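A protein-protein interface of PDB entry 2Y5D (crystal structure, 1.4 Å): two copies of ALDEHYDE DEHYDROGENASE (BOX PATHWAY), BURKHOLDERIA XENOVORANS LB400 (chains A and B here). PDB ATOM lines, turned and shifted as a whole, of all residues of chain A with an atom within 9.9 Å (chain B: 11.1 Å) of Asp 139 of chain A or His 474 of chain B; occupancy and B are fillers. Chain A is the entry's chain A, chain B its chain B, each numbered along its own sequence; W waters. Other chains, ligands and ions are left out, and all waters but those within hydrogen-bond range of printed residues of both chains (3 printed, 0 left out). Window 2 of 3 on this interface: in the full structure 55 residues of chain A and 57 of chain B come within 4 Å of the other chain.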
ATOM      1  N   SER A 135      28.633  10.038  26.733  1.00  0.00           N
ATOM      2  CA  SER A 135      27.629  10.567  25.782  1.00  0.00           C
ATOM      3  C   SER A 135      26.857   9.451  25.157  1.00  0.00           C
ATOM      4  O   SER A 135      27.397   8.430  24.799  1.00  0.00           O
ATOM      5  CB  SER A 135      28.386  11.352  24.647  1.00  0.00           C
ATOM      6  OG  SER A 135      27.374  11.973  23.808  1.00  0.00           O
ATOM      7  N   LEU A 136      25.547   9.730  25.033  1.00  0.00           N
ATOM      8  CA  LEU A 136      24.652   8.916  24.264  1.00  0.00           C
ATOM      9  C   LEU A 136      24.103   9.614  23.009  1.00  0.00           C
ATOM     10  O   LEU A 136      23.103   9.189  22.412  1.00  0.00           O
ATOM     11  CB  LEU A 136      23.466   8.528  25.148  1.00  0.00           C
ATOM     12  CG  LEU A 136      23.758   7.635  26.314  1.00  0.00           C
ATOM     13  CD1 LEU A 136      22.486   7.237  27.096  1.00  0.00           C
ATOM     14  CD2 LEU A 136      24.502   6.375  25.940  1.00  0.00           C
ATOM     15  N   SER A 137      24.726  10.678  22.544  1.00  0.00           N
ATOM     16  CA  SER A 137      24.212  11.437  21.400  1.00  0.00           C
ATOM     17  C   SER A 137      25.363  12.117  20.656  1.00  0.00           C
ATOM     18  O   SER A 137      26.270  12.570  21.274  1.00  0.00           O
ATOM     19  CB  SER A 137      23.239  12.568  21.851  1.00  0.00           C
ATOM     20  OG  SER A 137      23.735  13.308  22.984  1.00  0.00           O
ATOM     21  N   LYS A 138      25.193  12.243  19.331  1.00  0.00           N
ATOM     22  CA  LYS A 138      26.234  12.953  18.562  1.00  0.00           C
ATOM     23  C   LYS A 138      26.515  14.389  19.069  1.00  0.00           C
ATOM     24  O   LYS A 138      27.686  14.830  19.238  1.00  0.00           O
ATOM     25  CB  LYS A 138      25.872  12.929  17.059  1.00  0.00           C
ATOM     26  CG  LYS A 138      26.964  13.570  16.094  1.00  0.00           C
ATOM     27  CD  LYS A 138      28.048  12.477  15.750  1.00  0.00           C
ATOM     28  CE  LYS A 138      29.295  12.944  14.844  1.00  0.00           C
ATOM     29  NZ  LYS A 138      30.205  14.116  15.327  1.00  0.00           N
ATOM     30  N   ASP A 139      25.464  15.124  19.363  1.00  0.00           N
ATOM     31  CA  ASP A 139      25.608  16.506  19.874  1.00  0.00           C
ATOM     32  C   ASP A 139      25.877  16.638  21.366  1.00  0.00           C
ATOM     33  O   ASP A 139      25.893  17.760  21.873  1.00  0.00           O
ATOM     34  CB  ASP A 139      24.410  17.405  19.499  1.00  0.00           C
ATOM     35  CG  ASP A 139      23.105  17.023  20.197  1.00  0.00           C
ATOM     36  OD1 ASP A 139      23.116  16.163  21.111  1.00  0.00           O
ATOM     37  OD2 ASP A 139      22.105  17.702  19.911  1.00  0.00           O
ATOM     38  N   ARG A 140      25.999  15.493  22.079  1.00  0.00           N
ATOM     39  CA  ARG A 140      26.289  15.486  23.565  1.00  0.00           C
ATOM     40  C   ARG A 140      25.226  16.092  24.435  1.00  0.00           C
ATOM     41  O   ARG A 140      25.475  16.421  25.574  1.00  0.00           O
ATOM     42  CB  ARG A 140      27.659  16.215  23.842  1.00  0.00           C
ATOM     43  CG  ARG A 140      28.747  15.507  23.066  1.00  0.00           C
ATOM     44  CD  ARG A 140      30.127  16.208  23.314  1.00  0.00           C
ATOM     45  NE  ARG A 140      30.414  16.089  24.742  1.00  0.00           N
ATOM     46  CZ  ARG A 140      31.053  15.026  25.236  1.00  0.00           C
ATOM     47  NH1 ARG A 140      31.482  14.069  24.401  1.00  0.00           N
ATOM     48  NH2 ARG A 140      31.269  14.914  26.538  1.00  0.00           N
ATOM     49  N   SER A 141      23.972  16.222  23.940  1.00  0.00           N
ATOM     50  CA  SER A 141      22.886  16.814  24.731  1.00  0.00           C
ATOM     51  C   SER A 141      22.298  15.748  25.699  1.00  0.00           C
ATOM     52  O   SER A 141      21.716  16.108  26.701  1.00  0.00           O
ATOM     53  CB  SER A 141      21.735  17.329  23.789  1.00  0.00           C
ATOM     54  OG  SER A 141      21.272  16.285  22.946  1.00  0.00           O
ATOM     55  N   PHE A 142      22.505  14.493  25.309  1.00  0.00           N
ATOM     56  CA  PHE A 142      21.928  13.380  26.150  1.00  0.00           C
ATOM     57  C   PHE A 142      23.092  12.450  26.518  1.00  0.00           C
ATOM     58  O   PHE A 142      23.836  11.998  25.669  1.00  0.00           O
ATOM     59  CB  PHE A 142      20.920  12.619  25.348  1.00  0.00           C
ATOM     60  CG  PHE A 142      20.039  11.615  26.150  1.00  0.00           C
ATOM     61  CD1 PHE A 142      19.150  12.085  27.009  1.00  0.00           C
ATOM     62  CD2 PHE A 142      20.189  10.215  25.935  1.00  0.00           C
ATOM     63  CE1 PHE A 142      18.250  11.249  27.755  1.00  0.00           C
ATOM     64  CE2 PHE A 142      19.295   9.347  26.683  1.00  0.00           C
ATOM     65  CZ  PHE A 142      18.382   9.882  27.507  1.00  0.00           C
ATOM     66  N   SER A 143      23.252  12.157  27.828  1.00  0.00           N
ATOM     67  CA  SER A 143      24.373  11.372  28.332  1.00  0.00           C
ATOM     68  C   SER A 143      23.915  10.384  29.430  1.00  0.00           C
ATOM     69  O   SER A 143      22.768  10.396  29.857  1.00  0.00           O
ATOM     70  CB  SER A 143      25.366  12.380  29.069  1.00  0.00           C
ATOM     71  OG  SER A 143      25.968  13.052  27.950  1.00  0.00           O
ATOM     72  N   ALA A 517      20.080  11.073  30.825  1.00  0.00           N
ATOM     73  CA  ALA A 517      19.366  12.381  30.992  1.00  0.00           C
ATOM     74  C   ALA A 517      20.105  13.440  30.138  1.00  0.00           C
ATOM     75  O   ALA A 517      21.221  13.265  29.671  1.00  0.00           O
ATOM     76  CB  ALA A 517      19.309  12.827  32.448  1.00  0.00           C
ATOM     77  N   ALA A 518      19.406  14.576  30.018  1.00  0.00           N
ATOM     78  CA  ALA A 518      20.116  15.833  29.536  1.00  0.00           C
ATOM     79  C   ALA A 518      21.433  15.887  30.275  1.00  0.00           C
ATOM     80  O   ALA A 518      21.582  15.733  31.464  1.00  0.00           O
ATOM     81  CB  ALA A 518      19.263  16.988  29.831  1.00  0.00           C
ATOM     82  N   SER A 519      22.426  16.295  29.489  1.00  0.00           N
ATOM     83  CA  SER A 519      23.817  16.330  29.978  1.00  0.00           C
ATOM     84  C   SER A 519      24.016  17.285  31.161  1.00  0.00           C
ATOM     85  O   SER A 519      24.853  16.980  32.054  1.00  0.00           O
ATOM     86  CB  SER A 519      24.836  16.621  28.848  1.00  0.00           C
ATOM     87  OG  SER A 519      24.847  15.608  27.890  1.00  0.00           O
ATOM     88  N   ALA A 520      23.248  18.362  31.211  1.00  0.00           N
ATOM     89  CA  ALA A 520      23.353  19.272  32.381  1.00  0.00           C
ATOM     90  C   ALA A 520      22.946  18.552  33.670  1.00  0.00           C
ATOM     91  O   ALA A 520      23.698  18.699  34.677  1.00  0.00           O
ATOM     92  CB  ALA A 520      22.533  20.584  32.141  1.00  0.00           C
ATOM     93  N   PRO B 278       5.846  21.653  26.739  1.00  0.00           N
ATOM     94  CA  PRO B 278       6.447  20.751  25.772  1.00  0.00           C
ATOM     95  C   PRO B 278       6.676  19.325  26.362  1.00  0.00           C
ATOM     96  O   PRO B 278       6.624  18.352  25.623  1.00  0.00           O
ATOM     97  CB  PRO B 278       7.782  21.416  25.368  1.00  0.00           C
ATOM     98  CG  PRO B 278       7.619  22.823  25.813  1.00  0.00           C
ATOM     99  CD  PRO B 278       6.613  22.931  26.872  1.00  0.00           C
ATOM    100  N   LEU B 282       5.851  15.107  25.116  1.00  0.00           N
ATOM    101  CA  LEU B 282       6.910  14.038  25.039  1.00  0.00           C
ATOM    102  C   LEU B 282       6.475  12.852  25.883  1.00  0.00           C
ATOM    103  O   LEU B 282       6.693  11.708  25.403  1.00  0.00           O
ATOM    104  CB  LEU B 282       8.234  14.578  25.617  1.00  0.00           C
ATOM    105  CG  LEU B 282       8.802  15.839  24.917  1.00  0.00           C
ATOM    106  CD1 LEU B 282      10.117  16.223  25.589  1.00  0.00           C
ATOM    107  CD2 LEU B 282       8.995  15.541  23.438  1.00  0.00           C
ATOM    108  N   LYS B 285       3.764  10.900  23.866  1.00  0.00           N
ATOM    109  CA  LYS B 285       4.370  10.155  22.742  1.00  0.00           C
ATOM    110  C   LYS B 285       5.116   8.960  23.247  1.00  0.00           C
ATOM    111  O   LYS B 285       5.073   7.899  22.557  1.00  0.00           O
ATOM    112  CB  LYS B 285       5.326  11.045  21.940  1.00  0.00           C
ATOM    113  CG  LYS B 285       4.556  12.096  21.083  1.00  0.00           C
ATOM    114  CD  LYS B 285       5.393  12.269  19.796  1.00  0.00           C
ATOM    115  CE  LYS B 285       6.003  13.618  19.651  1.00  0.00           C
ATOM    116  NZ  LYS B 285       4.905  14.611  19.462  1.00  0.00           N
ATOM    117  N   GLU B 286       5.827   9.062  24.372  1.00  0.00           N
ATOM    118  CA  GLU B 286       6.689   7.942  24.818  1.00  0.00           C
ATOM    119  C   GLU B 286       5.776   6.833  25.340  1.00  0.00           C
ATOM    120  O   GLU B 286       6.097   5.630  25.053  1.00  0.00           O
ATOM    121  CB  GLU B 286       7.680   8.469  25.875  1.00  0.00           C
ATOM    122  CG  GLU B 286       8.897   7.542  26.010  1.00  0.00           C
ATOM    123  CD  GLU B 286       9.878   7.652  24.882  1.00  0.00           C
ATOM    124  OE1 GLU B 286       9.739   8.581  24.048  1.00  0.00           O
ATOM    125  OE2 GLU B 286      10.729   6.727  24.708  1.00  0.00           O
ATOM    126  N   ARG B 289       4.419   5.031  22.261  1.00  0.00           N
ATOM    127  CA  ARG B 289       5.459   4.214  21.583  1.00  0.00           C
ATOM    128  C   ARG B 289       5.747   2.959  22.398  1.00  0.00           C
ATOM    129  O   ARG B 289       5.903   1.843  21.755  1.00  0.00           O
ATOM    130  CB  ARG B 289       6.771   5.031  21.516  1.00  0.00           C
ATOM    131  CG  ARG B 289       7.807   4.508  20.615  1.00  0.00           C
ATOM    132  CD  ARG B 289       8.516   5.898  20.162  1.00  0.00           C
ATOM    133  NE  ARG B 289       9.873   6.084  20.703  1.00  0.00           N
ATOM    134  CZ  ARG B 289      10.479   7.250  21.066  1.00  0.00           C
ATOM    135  NH1 ARG B 289       9.855   8.423  21.067  1.00  0.00           N
ATOM    136  NH2 ARG B 289      11.750   7.219  21.494  1.00  0.00           N
ATOM    137  N   ASP B 448      15.451  20.640  33.356  1.00  0.00           N
ATOM    138  CA  ASP B 448      16.575  19.666  33.423  1.00  0.00           C
ATOM    139  C   ASP B 448      17.251  19.656  34.818  1.00  0.00           C
ATOM    140  O   ASP B 448      17.730  18.620  35.236  1.00  0.00           O
ATOM    141  CB  ASP B 448      17.646  19.994  32.359  1.00  0.00           C
ATOM    142  CG  ASP B 448      17.180  19.761  30.904  1.00  0.00           C
ATOM    143  OD1 ASP B 448      16.086  19.185  30.631  1.00  0.00           O
ATOM    144  OD2 ASP B 448      17.909  20.150  29.982  1.00  0.00           O
ATOM    145  N   HIS B 466      15.433   6.952  33.067  1.00  0.00           N
ATOM    146  CA  HIS B 466      15.541   7.537  31.702  1.00  0.00           C
ATOM    147  C   HIS B 466      14.757   8.852  31.728  1.00  0.00           C
ATOM    148  O   HIS B 466      13.548   8.896  31.848  1.00  0.00           O
ATOM    149  CB  HIS B 466      14.958   6.590  30.715  1.00  0.00           C
ATOM    150  CG  HIS B 466      15.228   7.045  29.354  1.00  0.00           C
ATOM    151  ND1 HIS B 466      14.299   7.677  28.550  1.00  0.00           N
ATOM    152  CD2 HIS B 466      16.322   6.863  28.610  1.00  0.00           C
ATOM    153  CE1 HIS B 466      14.856   7.919  27.363  1.00  0.00           C
ATOM    154  NE2 HIS B 466      16.110   7.437  27.412  1.00  0.00           N
ATOM    155  N   ALA B 467      15.519   9.970  31.649  1.00  0.00           N
ATOM    156  CA  ALA B 467      14.827  11.288  31.854  1.00  0.00           C
ATOM    157  C   ALA B 467      14.674  11.964  30.505  1.00  0.00           C
ATOM    158  O   ALA B 467      15.640  12.196  29.752  1.00  0.00           O
ATOM    159  CB  ALA B 467      15.623  12.093  32.730  1.00  0.00           C
ATOM    160  N   ILE B 468      13.437  12.215  30.153  1.00  0.00           N
ATOM    161  CA  ILE B 468      13.078  12.927  28.877  1.00  0.00           C
ATOM    162  C   ILE B 468      12.535  14.395  29.170  1.00  0.00           C
ATOM    163  O   ILE B 468      11.726  14.660  30.045  1.00  0.00           O
ATOM    164  CB  ILE B 468      11.948  12.135  28.189  1.00  0.00           C
ATOM    165  CG1 ILE B 468      12.575  10.807  27.712  1.00  0.00           C
ATOM    166  CG2 ILE B 468      11.350  12.881  26.966  1.00  0.00           C
ATOM    167  CD1 ILE B 468      11.532   9.703  27.301  1.00  0.00           C
ATOM    168  N   SER B 469      13.168  15.322  28.428  1.00  0.00           N
ATOM    169  CA  SER B 469      12.800  16.745  28.625  1.00  0.00           C
ATOM    170  C   SER B 469      13.031  17.369  27.260  1.00  0.00           C
ATOM    171  O   SER B 469      13.649  16.830  26.384  1.00  0.00           O
ATOM    172  CB  SER B 469      13.711  17.300  29.678  1.00  0.00           C
ATOM    173  OG  SER B 469      15.123  17.204  29.313  1.00  0.00           O
ATOM    174  N   PRO B 470      12.537  18.631  27.095  1.00  0.00           N
ATOM    175  CA  PRO B 470      12.674  19.277  25.813  1.00  0.00           C
ATOM    176  C   PRO B 470      14.093  19.415  25.199  1.00  0.00           C
ATOM    177  O   PRO B 470      14.241  19.221  23.954  1.00  0.00           O
ATOM    178  CB  PRO B 470      12.007  20.632  26.063  1.00  0.00           C
ATOM    179  CG  PRO B 470      10.954  20.361  27.162  1.00  0.00           C
ATOM    180  CD  PRO B 470      11.697  19.359  28.065  1.00  0.00           C
ATOM    181  N   SER B 471      15.093  19.662  26.055  1.00  0.00           N
ATOM    182  CA  SER B 471      16.411  19.782  25.473  1.00  0.00           C
ATOM    183  C   SER B 471      16.923  18.508  24.831  1.00  0.00           C
ATOM    184  O   SER B 471      17.896  18.544  24.110  1.00  0.00           O
ATOM    185  CB  SER B 471      17.415  20.247  26.483  1.00  0.00           C
ATOM    186  OG  SER B 471      17.745  19.164  27.446  1.00  0.00           O
ATOM    187  N   VAL B 472      16.330  17.345  25.169  1.00  0.00           N
ATOM    188  CA  VAL B 472      16.741  16.067  24.539  1.00  0.00           C
ATOM    189  C   VAL B 472      15.571  15.489  23.766  1.00  0.00           C
ATOM    190  O   VAL B 472      15.568  14.251  23.458  1.00  0.00           O
ATOM    191  CB  VAL B 472      17.302  15.094  25.630  1.00  0.00           C
ATOM    192  CG1 VAL B 472      18.624  15.717  26.138  1.00  0.00           C
ATOM    193  CG2 VAL B 472      16.231  14.693  26.760  1.00  0.00           C
ATOM    194  N   GLN B 473      14.631  16.294  23.229  1.00  0.00           N
ATOM    195  CA  GLN B 473      13.547  15.682  22.460  1.00  0.00           C
ATOM    196  C   GLN B 473      14.077  14.896  21.247  1.00  0.00           C
ATOM    197  O   GLN B 473      13.515  13.915  20.850  1.00  0.00           O
ATOM    198  CB  GLN B 473      12.515  16.754  22.027  1.00  0.00           C
ATOM    199  CG  GLN B 473      13.120  17.803  21.131  1.00  0.00           C
ATOM    200  CD  GLN B 473      11.986  18.783  20.663  1.00  0.00           C
ATOM    201  OE1 GLN B 473      10.768  18.552  20.929  1.00  0.00           O
ATOM    202  NE2 GLN B 473      12.394  19.893  19.998  1.00  0.00           N
ATOM    203  N   HIS B 474      15.152  15.372  20.647  1.00  0.00           N
ATOM    204  CA  HIS B 474      15.720  14.823  19.436  1.00  0.00           C
ATOM    205  C   HIS B 474      16.835  13.778  19.664  1.00  0.00           C
ATOM    206  O   HIS B 474      17.281  13.096  18.751  1.00  0.00           O
ATOM    207  CB  HIS B 474      16.325  16.064  18.687  1.00  0.00           C
ATOM    208  CG  HIS B 474      17.513  16.635  19.428  1.00  0.00           C
ATOM    209  ND1 HIS B 474      17.482  17.182  20.732  1.00  0.00           N
ATOM    210  CD2 HIS B 474      18.822  16.615  19.052  1.00  0.00           C
ATOM    211  CE1 HIS B 474      18.731  17.508  21.053  1.00  0.00           C
ATOM    212  NE2 HIS B 474      19.550  17.146  20.054  1.00  0.00           N
ATOM    213  N   SER B 475      17.364  13.729  20.870  1.00  0.00           N
ATOM    214  CA  SER B 475      18.546  12.899  21.217  1.00  0.00           C
ATOM    215  C   SER B 475      18.229  11.771  22.207  1.00  0.00           C
ATOM    216  O   SER B 475      19.015  10.880  22.249  1.00  0.00           O
ATOM    217  CB  SER B 475      19.697  13.795  21.760  1.00  0.00           C
ATOM    218  OG  SER B 475      19.235  14.549  22.857  1.00  0.00           O
ATOM    219  N   GLN B 476      17.222  11.934  23.045  1.00  0.00           N
ATOM    220  CA  GLN B 476      16.959  10.883  24.057  1.00  0.00           C
ATOM    221  C   GLN B 476      16.699   9.515  23.295  1.00  0.00           C
ATOM    222  O   GLN B 476      16.055   9.464  22.252  1.00  0.00           O
ATOM    223  CB  GLN B 476      15.734  11.226  24.924  1.00  0.00           C
ATOM    224  CG  GLN B 476      14.428  11.319  24.203  1.00  0.00           C
ATOM    225  CD  GLN B 476      13.597  10.054  24.330  1.00  0.00           C
ATOM    226  OE1 GLN B 476      14.017   9.079  24.940  1.00  0.00           O
ATOM    227  NE2 GLN B 476      12.423  10.105  23.791  1.00  0.00           N
ATOM    228  N   THR B 477      17.276   8.441  23.885  1.00  0.00           N
ATOM    229  CA  THR B 477      17.402   7.191  23.173  1.00  0.00           C
ATOM    230  C   THR B 477      16.178   6.262  23.388  1.00  0.00           C
ATOM    231  O   THR B 477      16.217   5.160  22.818  1.00  0.00           O
ATOM    232  CB  THR B 477      18.666   6.471  23.622  1.00  0.00           C
ATOM    233  OG1 THR B 477      18.770   6.428  25.030  1.00  0.00           O
ATOM    234  CG2 THR B 477      19.939   7.232  23.012  1.00  0.00           C
ATOM    235  N   GLY B 478      15.153   6.686  24.098  1.00  0.00           N
ATOM    236  CA  GLY B 478      13.910   5.840  24.244  1.00  0.00           C
ATOM    237  C   GLY B 478      13.850   5.236  25.618  1.00  0.00           C
ATOM    238  O   GLY B 478      14.806   4.647  26.131  1.00  0.00           O
ATOM    239  N   ASN B 481      14.316   1.305  24.857  1.00  0.00           N
ATOM    240  CA  ASN B 481      15.461   0.862  24.073  1.00  0.00           C
ATOM    241  C   ASN B 481      16.673   0.738  24.939  1.00  0.00           C
ATOM    242  O   ASN B 481      16.896   1.599  25.832  1.00  0.00           O
ATOM    243  CB  ASN B 481      15.702   1.889  22.986  1.00  0.00           C
ATOM    244  CG  ASN B 481      14.619   1.901  21.987  1.00  0.00           C
ATOM    245  OD1 ASN B 481      14.082   0.842  21.584  1.00  0.00           O
ATOM    246  ND2 ASN B 481      14.237   3.112  21.573  1.00  0.00           N
ATOM    247  N   MET B 483      20.355   0.757  25.477  1.00  0.00           N
ATOM    248  CA  MET B 483      21.631   1.133  24.939  1.00  0.00           C
ATOM    249  C   MET B 483      22.733   0.275  25.571  1.00  0.00           C
ATOM    250  O   MET B 483      22.796   0.153  26.771  1.00  0.00           O
ATOM    251  CB  MET B 483      21.924   2.638  25.183  1.00  0.00           C
ATOM    252  CG  MET B 483      20.923   3.617  24.546  1.00  0.00           C
ATOM    253  SD  MET B 483      20.897   3.443  22.755  1.00  0.00           S
ATOM    254  CE  MET B 483      19.472   2.357  22.497  1.00  0.00           C
HETATM  255  O   HOH W   1      20.460  18.676  27.063  1.00  0.00           O
HETATM  256  O   HOH W   2      16.599  14.783  30.306  1.00  0.00           O
HETATM  257  O   HOH W   3      21.123   9.996  20.759  1.00  0.00           O
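Of the 13 printed residues of chain A, 7 touch a printed residue of chain B. Hydrophobic or aromatic side chains of chain A within 4 Å of the printed part of chain B: Phe 142, Ala 517 and Ala 518. Among the printed residues, no Asp or Glu carboxylate lies within 4 Å of a Lys or Arg side-chain nitrogen of the other chain.
OE1 of Glu 286 of chain B lies within hydrogen-bond range of NE2 of Gln 476 of chain B. The backbone carbonyl oxygen of Ser 143 of chain A lies within hydrogen-bond range of the backbone NH of Ala 517 of chain A, 2.9 Å away. OD1 of Asp 139 of chain A is in hydrogen-bond range of OG of Ser 141 of chain A. O of Phe 142 of chain A lies within hydrogen-bond range of N of Leu 136 of chain A. O of Ser 137 of chain A is in hydrogen-bond range of OG of Ser 135 of chain A (2.8 Å). OD1 of Asp 448 of chain B lies within hydrogen-bond range of OG of Ser 469 of chain B.
Among the printed residues, merely in contact across the chains: Leu 136 of chain A with Thr 477 of chain B, Ser 137 of chain A with Ser 475 of chain B, Ser 141 of chain A with Val 472 of chain B, Phe 142 of chain A with His 466 of chain B, Phe 142 of chain A with Ala 467 of chain B, Phe 142 of chain A with Val 472 of chain B, Phe 142 of chain A with Ser 475 of chain B, Phe 142 of chain A with Gln 476 of chain B, Phe 142 of chain A with Thr 477 of chain B, Ala 517 of chain A with Ala 467 of chain B, Ala 518 of chain A with Asp 448 of chain B, Ala 518 of chain A with Ser 471 of chain B and Ala 518 of chain A with Val 472 of chain B.
Of chain B, only Ser 475 (3.7 Å) comes within 4 Å of Ser 137 of chain A. No residue of chain B comes within 4 Å of Lys 138 of chain A. Printed residues of chain B within 4 Å of Asp 139 of chain A: His 474. Ser 141 of chain A touches three residues of chain B. Of the printed residues of chain B, Ala 517 of chain A touches Ala 467 (3.8 Å). Printed residues of chain B within 4 Å of Ala 518 of chain A: Asp 448, Ser 471 and Val 472. Of the printed residues of chain A, His 466 of chain B touches Phe 142 (3.3 Å). Of chain A, only Asp 139 and Ser 141 come within 4 Å of His 474 of chain B. Ser 475 of chain B touches three residues of chain A. Printed residues of chain A within 4 Å of Thr 477 of chain B: Leu 136 (3.8 Å) and Phe 142 (3.4 Å). Gly 478 of chain B touches none of the printed residues of chain A. The nearest residue of chain B that does not touch Asp 139 of chain A is Ser 475 of chain B (4.2 Å). The nearest printed residue of chain A that does not touch Val 472 of chain B is Ala 517 of chain A (4.8 Å).
The side-chain hydroxyl (OG) of Ser 141 of chain A sits close to a ring nitrogen (NE2) of His 474 of chain B. OD2 of Asp 139 of chain A sits at hydrogen-bond distance from NE2 of His 474 of chain B (2.6 Å). The side-chain hydroxyl (OG) of Ser 141 of chain A sits at hydrogen-bond distance from the side-chain hydroxyl (OG) of Ser 475 of chain B, 2.7 Å away.
Water W3 bridges O of Leu 136 of chain A and O of Ser 475 of chain B. Water W1 lies within hydrogen-bond range of the side-chain hydroxyl (OG) of Ser 471 of chain B (2.8 Å) and the backbone carbonyl oxygen (O) of Ser 141 of chain A (2.9 Å). Water W2 lies within hydrogen-bond range of the backbone carbonyl oxygen of Ala 467 of chain B (2.8 Å), the backbone NH of Ala 518 of chain A (2.8 Å) and the side-chain hydroxyl of Ser 469 of chain B (3.0 Å).
No position is printed for both chains. Of the 16 pairs that touch across the chains among the printed residues, none has its exchanged pair printed and touching as well.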
